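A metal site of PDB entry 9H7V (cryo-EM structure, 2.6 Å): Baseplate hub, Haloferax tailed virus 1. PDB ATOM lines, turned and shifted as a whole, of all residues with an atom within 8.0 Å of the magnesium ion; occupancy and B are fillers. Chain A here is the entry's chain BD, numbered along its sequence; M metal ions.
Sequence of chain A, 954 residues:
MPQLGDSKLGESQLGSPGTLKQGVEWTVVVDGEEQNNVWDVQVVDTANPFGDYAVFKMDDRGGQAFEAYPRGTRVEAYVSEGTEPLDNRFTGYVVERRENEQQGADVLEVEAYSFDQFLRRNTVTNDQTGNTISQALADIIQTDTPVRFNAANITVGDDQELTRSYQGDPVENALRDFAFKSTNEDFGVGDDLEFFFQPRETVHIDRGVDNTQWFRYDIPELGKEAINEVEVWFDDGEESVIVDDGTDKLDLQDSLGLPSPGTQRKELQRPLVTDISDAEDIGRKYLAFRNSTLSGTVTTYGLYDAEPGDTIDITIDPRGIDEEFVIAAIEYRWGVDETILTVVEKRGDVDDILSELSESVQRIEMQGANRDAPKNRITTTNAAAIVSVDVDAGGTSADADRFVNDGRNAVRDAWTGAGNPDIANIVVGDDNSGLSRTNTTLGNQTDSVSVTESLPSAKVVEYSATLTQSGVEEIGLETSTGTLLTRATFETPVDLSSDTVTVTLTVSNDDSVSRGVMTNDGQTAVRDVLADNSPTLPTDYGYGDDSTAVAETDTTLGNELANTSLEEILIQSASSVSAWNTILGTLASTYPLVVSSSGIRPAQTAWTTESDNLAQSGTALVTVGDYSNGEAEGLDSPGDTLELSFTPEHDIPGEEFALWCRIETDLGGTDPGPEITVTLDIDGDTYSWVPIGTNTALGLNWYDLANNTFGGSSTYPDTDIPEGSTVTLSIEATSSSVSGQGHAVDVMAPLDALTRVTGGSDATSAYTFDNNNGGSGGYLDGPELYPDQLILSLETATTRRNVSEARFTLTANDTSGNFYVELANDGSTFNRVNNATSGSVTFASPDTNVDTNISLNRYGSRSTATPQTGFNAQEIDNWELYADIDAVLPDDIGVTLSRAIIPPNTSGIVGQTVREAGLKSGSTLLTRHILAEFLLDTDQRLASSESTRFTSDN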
ATOM      1  N   THR A 609     -18.386  11.183  30.189  1.00  0.00           N
ATOM      2  CA  THR A 609     -18.820   9.799  30.337  1.00  0.00           C
ATOM      3  C   THR A 609     -20.327   9.708  30.098  1.00  0.00           C
ATOM      4  O   THR A 609     -21.100  10.457  30.684  1.00  0.00           O
ATOM      5  CB  THR A 609     -18.410   9.228  31.698  1.00  0.00           C
ATOM      6  OG1 THR A 609     -17.010   9.480  31.877  1.00  0.00           O
ATOM      7  CG2 THR A 609     -18.669   7.746  31.827  1.00  0.00           C
ATOM      8  N   GLU A 610     -20.699   8.745  29.249  1.00  0.00           N
ATOM      9  CA  GLU A 610     -22.063   8.451  28.873  1.00  0.00           C
ATOM     10  C   GLU A 610     -22.786   7.785  30.049  1.00  0.00           C
ATOM     11  O   GLU A 610     -22.140   7.225  30.937  1.00  0.00           O
ATOM     12  CB  GLU A 610     -22.021   7.539  27.635  1.00  0.00           C
ATOM     13  CG  GLU A 610     -23.353   7.329  26.942  1.00  0.00           C
ATOM     14  CD  GLU A 610     -24.220   8.565  26.798  1.00  0.00           C
ATOM     15  OE1 GLU A 610     -23.801   9.503  26.108  1.00  0.00           O
ATOM     16  OE2 GLU A 610     -25.309   8.580  27.403  1.00  0.00           O
ATOM     17  N   SER A 611     -24.125   7.862  30.023  1.00  0.00           N
ATOM     18  CA  SER A 611     -25.025   7.289  31.016  1.00  0.00           C
ATOM     19  C   SER A 611     -24.692   5.833  31.318  1.00  0.00           C
ATOM     20  O   SER A 611     -24.511   5.478  32.480  1.00  0.00           O
ATOM     21  CB  SER A 611     -26.458   7.426  30.555  1.00  0.00           C
ATOM     22  OG  SER A 611     -26.636   6.932  29.244  1.00  0.00           O
ATOM     23  N   ASP A 612     -24.611   5.003  30.261  1.00  0.00           N
ATOM     24  CA  ASP A 612     -24.530   3.559  30.366  1.00  0.00           C
ATOM     25  C   ASP A 612     -23.149   3.114  30.861  1.00  0.00           C
ATOM     26  O   ASP A 612     -22.948   1.934  31.162  1.00  0.00           O
ATOM     27  CB  ASP A 612     -24.893   2.885  29.035  1.00  0.00           C
ATOM     28  CG  ASP A 612     -23.981   3.274  27.883  1.00  0.00           C
ATOM     29  OD1 ASP A 612     -22.880   2.702  27.778  1.00  0.00           O
ATOM     30  OD2 ASP A 612     -24.380   4.160  27.106  1.00  0.00           O
ATOM     31  N   ASN A 613     -22.209   4.067  30.953  1.00  0.00           N
ATOM     32  CA  ASN A 613     -20.807   3.793  31.230  1.00  0.00           C
ATOM     33  C   ASN A 613     -20.480   4.070  32.706  1.00  0.00           C
ATOM     34  O   ASN A 613     -19.442   3.630  33.198  1.00  0.00           O
ATOM     35  CB  ASN A 613     -19.896   4.551  30.267  1.00  0.00           C
ATOM     36  CG  ASN A 613     -18.637   3.813  29.877  1.00  0.00           C
ATOM     37  OD1 ASN A 613     -18.287   3.752  28.704  1.00  0.00           O
ATOM     38  ND2 ASN A 613     -17.929   3.243  30.853  1.00  0.00           N
ATOM     39  N   VAL A 622     -33.683   5.023  31.884  1.00  0.00           N
ATOM     40  CA  VAL A 622     -34.584   5.979  31.263  1.00  0.00           C
ATOM     41  C   VAL A 622     -34.245   6.083  29.770  1.00  0.00           C
ATOM     42  O   VAL A 622     -33.096   6.348  29.432  1.00  0.00           O
ATOM     43  CB  VAL A 622     -34.540   7.350  31.963  1.00  0.00           C
ATOM     44  CG1 VAL A 622     -35.398   8.393  31.269  1.00  0.00           C
ATOM     45  CG2 VAL A 622     -34.907   7.258  33.433  1.00  0.00           C
ATOM     46  N   VAL A 624     -35.311   8.051  26.272  1.00  0.00           N
ATOM     47  CA  VAL A 624     -35.931   9.048  25.409  1.00  0.00           C
ATOM     48  C   VAL A 624     -34.919   9.398  24.314  1.00  0.00           C
ATOM     49  O   VAL A 624     -33.724   9.510  24.601  1.00  0.00           O
ATOM     50  CB  VAL A 624     -36.377  10.317  26.164  1.00  0.00           C
ATOM     51  CG1 VAL A 624     -37.287  11.204  25.320  1.00  0.00           C
ATOM     52  CG2 VAL A 624     -37.034  10.044  27.515  1.00  0.00           C
ATOM     53  N   ASP A 626     -33.958  11.955  22.609  1.00  0.00           N
ATOM     54  CA  ASP A 626     -33.142  13.160  22.625  1.00  0.00           C
ATOM     55  C   ASP A 626     -32.089  13.135  23.731  1.00  0.00           C
ATOM     56  O   ASP A 626     -31.315  14.085  23.867  1.00  0.00           O
ATOM     57  CB  ASP A 626     -33.975  14.455  22.533  1.00  0.00           C
ATOM     58  CG  ASP A 626     -35.058  14.620  23.589  1.00  0.00           C
ATOM     59  OD1 ASP A 626     -35.278  13.674  24.379  1.00  0.00           O
ATOM     60  OD2 ASP A 626     -35.680  15.702  23.612  1.00  0.00           O
ATOM     61  N   TYR A 627     -32.054  12.044  24.512  1.00  0.00           N
ATOM     62  CA  TYR A 627     -30.925  11.777  25.386  1.00  0.00           C
ATOM     63  C   TYR A 627     -29.804  11.134  24.572  1.00  0.00           C
ATOM     64  O   TYR A 627     -30.061  10.457  23.580  1.00  0.00           O
ATOM     65  CB  TYR A 627     -31.336  10.922  26.590  1.00  0.00           C
ATOM     66  CG  TYR A 627     -32.312  11.525  27.566  1.00  0.00           C
ATOM     67  CD1 TYR A 627     -32.502  12.901  27.673  1.00  0.00           C
ATOM     68  CD2 TYR A 627     -33.053  10.709  28.417  1.00  0.00           C
ATOM     69  CE1 TYR A 627     -33.402  13.440  28.580  1.00  0.00           C
ATOM     70  CE2 TYR A 627     -33.948  11.233  29.337  1.00  0.00           C
ATOM     71  CZ  TYR A 627     -34.126  12.612  29.412  1.00  0.00           C
ATOM     72  OH  TYR A 627     -35.012  13.124  30.316  1.00  0.00           O
ATOM     73  N   SER A 628     -28.551  11.398  24.987  1.00  0.00           N
ATOM     74  CA  SER A 628     -27.354  10.833  24.383  1.00  0.00           C
ATOM     75  C   SER A 628     -27.311   9.329  24.603  1.00  0.00           C
ATOM     76  O   SER A 628     -27.419   8.873  25.748  1.00  0.00           O
ATOM     77  CB  SER A 628     -26.103  11.475  24.936  1.00  0.00           C
ATOM     78  OG  SER A 628     -26.223  12.891  25.013  1.00  0.00           O
ATOM     79  N   ASN A 629     -27.117   8.617  23.480  1.00  0.00           N
ATOM     80  CA  ASN A 629     -27.184   7.167  23.328  1.00  0.00           C
ATOM     81  C   ASN A 629     -28.628   6.699  23.510  1.00  0.00           C
ATOM     82  O   ASN A 629     -28.892   5.505  23.711  1.00  0.00           O
ATOM     83  CB  ASN A 629     -26.149   6.424  24.177  1.00  0.00           C
ATOM     84  CG  ASN A 629     -25.882   4.996  23.726  1.00  0.00           C
ATOM     85  OD1 ASN A 629     -26.080   4.656  22.560  1.00  0.00           O
ATOM     86  ND2 ASN A 629     -25.429   4.153  24.637  1.00  0.00           N
ATOM     87  N   GLY A 630     -29.562   7.652  23.447  1.00  0.00           N
ATOM     88  CA  GLY A 630     -30.986   7.394  23.622  1.00  0.00           C
ATOM     89  C   GLY A 630     -31.373   7.122  25.072  1.00  0.00           C
ATOM     90  O   GLY A 630     -32.529   6.781  25.330  1.00  0.00           O
ATOM     91  N   GLU A 631     -30.424   7.264  26.001  1.00  0.00           N
ATOM     92  CA  GLU A 631     -30.662   6.851  27.379  1.00  0.00           C
ATOM     93  C   GLU A 631     -29.893   7.693  28.406  1.00  0.00           C
ATOM     94  O   GLU A 631     -28.869   8.312  28.103  1.00  0.00           O
ATOM     95  CB  GLU A 631     -30.483   5.338  27.554  1.00  0.00           C
ATOM     96  CG  GLU A 631     -29.046   4.852  27.435  1.00  0.00           C
ATOM     97  CD  GLU A 631     -28.918   3.351  27.245  1.00  0.00           C
ATOM     98  OE1 GLU A 631     -29.391   2.833  26.217  1.00  0.00           O
ATOM     99  OE2 GLU A 631     -28.357   2.693  28.150  1.00  0.00           O
ATOM    100  N   ALA A 632     -30.449   7.668  29.623  1.00  0.00           N
ATOM    101  CA  ALA A 632     -29.986   8.406  30.789  1.00  0.00           C
ATOM    102  C   ALA A 632     -30.278   7.599  32.047  1.00  0.00           C
ATOM    103  O   ALA A 632     -31.073   6.648  32.009  1.00  0.00           O
ATOM    104  CB  ALA A 632     -30.691   9.754  30.843  1.00  0.00           C
ATOM    105  N   GLU A 633     -29.632   7.971  33.157  1.00  0.00           N
ATOM    106  CA  GLU A 633     -29.804   7.286  34.428  1.00  0.00           C
ATOM    107  C   GLU A 633     -30.703   8.124  35.341  1.00  0.00           C
ATOM    108  O   GLU A 633     -30.394   9.286  35.607  1.00  0.00           O
ATOM    109  CB  GLU A 633     -28.458   6.986  35.093  1.00  0.00           C
ATOM    110  CG  GLU A 633     -27.486   6.212  34.223  1.00  0.00           C
ATOM    111  CD  GLU A 633     -27.948   4.890  33.625  1.00  0.00           C
ATOM    112  OE1 GLU A 633     -28.850   4.245  34.190  1.00  0.00           O
ATOM    113  OE2 GLU A 633     -27.380   4.501  32.578  1.00  0.00           O
ATOM    114  N   ARG A 662     -25.528  16.924  31.788  1.00  0.00           N
ATOM    115  CA  ARG A 662     -26.728  17.058  30.978  1.00  0.00           C
ATOM    116  C   ARG A 662     -27.839  16.293  31.688  1.00  0.00           C
ATOM    117  O   ARG A 662     -27.806  15.059  31.750  1.00  0.00           O
ATOM    118  CB  ARG A 662     -26.478  16.575  29.550  1.00  0.00           C
ATOM    119  CG  ARG A 662     -27.619  16.874  28.593  1.00  0.00           C
ATOM    120  CD  ARG A 662     -27.248  16.550  27.156  1.00  0.00           C
ATOM    121  NE  ARG A 662     -28.209  17.142  26.223  1.00  0.00           N
ATOM    122  CZ  ARG A 662     -29.039  16.466  25.445  1.00  0.00           C
ATOM    123  NH1 ARG A 662     -29.857  17.128  24.641  1.00  0.00           N
ATOM    124  NH2 ARG A 662     -29.060  15.143  25.444  1.00  0.00           N
ATOM    125  N   VAL A 745     -29.906  11.851  34.391  1.00  0.00           N
ATOM    126  CA  VAL A 745     -28.631  12.388  33.952  1.00  0.00           C
ATOM    127  C   VAL A 745     -28.141  11.576  32.746  1.00  0.00           C
ATOM    128  O   VAL A 745     -28.073  10.354  32.793  1.00  0.00           O
ATOM    129  CB  VAL A 745     -27.591  12.502  35.092  1.00  0.00           C
ATOM    130  CG1 VAL A 745     -27.251  11.166  35.735  1.00  0.00           C
ATOM    131  CG2 VAL A 745     -26.331  13.244  34.667  1.00  0.00           C
ATOM    132  N   ASP A 746     -27.785  12.309  31.689  1.00  0.00           N
ATOM    133  CA  ASP A 746     -27.688  11.789  30.338  1.00  0.00           C
ATOM    134  C   ASP A 746     -26.231  11.490  29.957  1.00  0.00           C
ATOM    135  O   ASP A 746     -25.991  10.583  29.153  1.00  0.00           O
ATOM    136  CB  ASP A 746     -28.311  12.770  29.352  1.00  0.00           C
ATOM    137  CG  ASP A 746     -28.132  12.373  27.891  1.00  0.00           C
ATOM    138  OD1 ASP A 746     -28.286  11.168  27.597  1.00  0.00           O
ATOM    139  OD2 ASP A 746     -27.859  13.269  27.074  1.00  0.00           O
ATOM    140  N   VAL A 747     -25.330  12.329  30.505  1.00  0.00           N
ATOM    141  CA  VAL A 747     -23.889  12.362  30.308  1.00  0.00           C
ATOM    142  C   VAL A 747     -23.268  13.253  31.398  1.00  0.00           C
ATOM    143  O   VAL A 747     -23.802  14.317  31.720  1.00  0.00           O
ATOM    144  CB  VAL A 747     -23.489  12.798  28.880  1.00  0.00           C
ATOM    145  CG1 VAL A 747     -24.238  14.018  28.369  1.00  0.00           C
ATOM    146  CG2 VAL A 747     -21.986  12.961  28.679  1.00  0.00           C
ATOM    147  N   MET A 748     -22.138  12.786  31.963  1.00  0.00           N
ATOM    148  CA  MET A 748     -21.415  13.485  33.019  1.00  0.00           C
ATOM    149  C   MET A 748     -20.053  13.937  32.500  1.00  0.00           C
ATOM    150  O   MET A 748     -19.319  13.155  31.908  1.00  0.00           O
ATOM    151  CB  MET A 748     -21.207  12.560  34.222  1.00  0.00           C
ATOM    152  CG  MET A 748     -22.336  12.607  35.228  1.00  0.00           C
ATOM    153  SD  MET A 748     -21.714  12.754  36.925  1.00  0.00           S
ATOM    154  CE  MET A 748     -21.060  11.105  37.203  1.00  0.00           C
ATOM    155  N   ASN A 773     -29.171  16.252  19.724  1.00  0.00           N
ATOM    156  CA  ASN A 773     -28.629  15.063  19.079  1.00  0.00           C
ATOM    157  C   ASN A 773     -29.508  14.621  17.904  1.00  0.00           C
ATOM    158  O   ASN A 773     -29.239  13.587  17.287  1.00  0.00           O
ATOM    159  CB  ASN A 773     -28.422  13.919  20.089  1.00  0.00           C
ATOM    160  CG  ASN A 773     -29.727  13.304  20.578  1.00  0.00           C
ATOM    161  OD1 ASN A 773     -30.765  13.961  20.598  1.00  0.00           O
ATOM    162  ND2 ASN A 773     -29.670  12.043  20.967  1.00  0.00           N
ATOM    163  N   GLY A 778     -29.469   9.437  19.181  1.00  0.00           N
ATOM    164  CA  GLY A 778     -28.154   9.728  18.626  1.00  0.00           C
ATOM    165  C   GLY A 778     -27.136  10.165  19.683  1.00  0.00           C
ATOM    166  O   GLY A 778     -27.449  10.216  20.877  1.00  0.00           O
ATOM    167  N   TYR A 779     -25.929  10.460  19.203  1.00  0.00           N
ATOM    168  CA  TYR A 779     -24.811  10.921  20.021  1.00  0.00           C
ATOM    169  C   TYR A 779     -24.666  12.440  19.868  1.00  0.00           C
ATOM    170  O   TYR A 779     -25.337  13.043  19.037  1.00  0.00           O
ATOM    171  CB  TYR A 779     -23.547  10.116  19.709  1.00  0.00           C
ATOM    172  CG  TYR A 779     -23.750   8.633  19.862  1.00  0.00           C
ATOM    173  CD1 TYR A 779     -23.669   8.025  21.107  1.00  0.00           C
ATOM    174  CD2 TYR A 779     -24.053   7.833  18.768  1.00  0.00           C
ATOM    175  CE1 TYR A 779     -23.867   6.657  21.260  1.00  0.00           C
ATOM    176  CE2 TYR A 779     -24.254   6.465  18.908  1.00  0.00           C
ATOM    177  CZ  TYR A 779     -24.155   5.881  20.157  1.00  0.00           C
ATOM    178  OH  TYR A 779     -24.357   4.534  20.305  1.00  0.00           O
ATOM    179  N   THR A 866     -20.245   9.591  22.405  1.00  0.00           N
ATOM    180  CA  THR A 866     -20.010  10.931  22.923  1.00  0.00           C
ATOM    181  C   THR A 866     -18.608  11.005  23.518  1.00  0.00           C
ATOM    182  O   THR A 866     -18.162  10.033  24.123  1.00  0.00           O
ATOM    183  CB  THR A 866     -21.019  11.295  24.017  1.00  0.00           C
ATOM    184  OG1 THR A 866     -21.107  10.217  24.950  1.00  0.00           O
ATOM    185  CG2 THR A 866     -22.395  11.629  23.475  1.00  0.00           C
HETATM  186 MG    MG M   1     -27.180   9.279  27.703  1.00  0.00          MG
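Ser 611 touches the magnesium ion. Of the 24 residues printed, 5 come within 4 Å of the magnesium ion. The nearest printed residue that does not touch the magnesium ion is Ala 632 (4.1 Å).
The magnesium ion is bound by the backbone carbonyl oxygen (O) of Glu 631, the backbone carbonyl oxygen (O) of Ser 628, the side-chain carboxylate (OE2) of Glu 610, the side-chain carboxylate (OD1) of Asp 746 and the backbone carbonyl oxygen (O) of Asp 746. The magnesium ion has five donor atoms within binding distance.
The side-chain carboxylate (OE2) of Glu 610 lies close to the side-chain hydroxyl (OG) of Ser 611 (2.8 Å). OG1 of Thr 866 sits at hydrogen-bond distance from OE1 of Glu 610, 3.0 Å away. The backbone NH (N) of Ser 611 lies close to the backbone carbonyl oxygen (O) of Asp 746, 3.4 Å away. O of Glu 631 lies close to OG of Ser 611 (2.9 Å). The side-chain carboxylate (OD2) of Asp 746 lies within salt-bridge range of the guanidinium group (NH2) of Arg 662 (2.8 Å).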
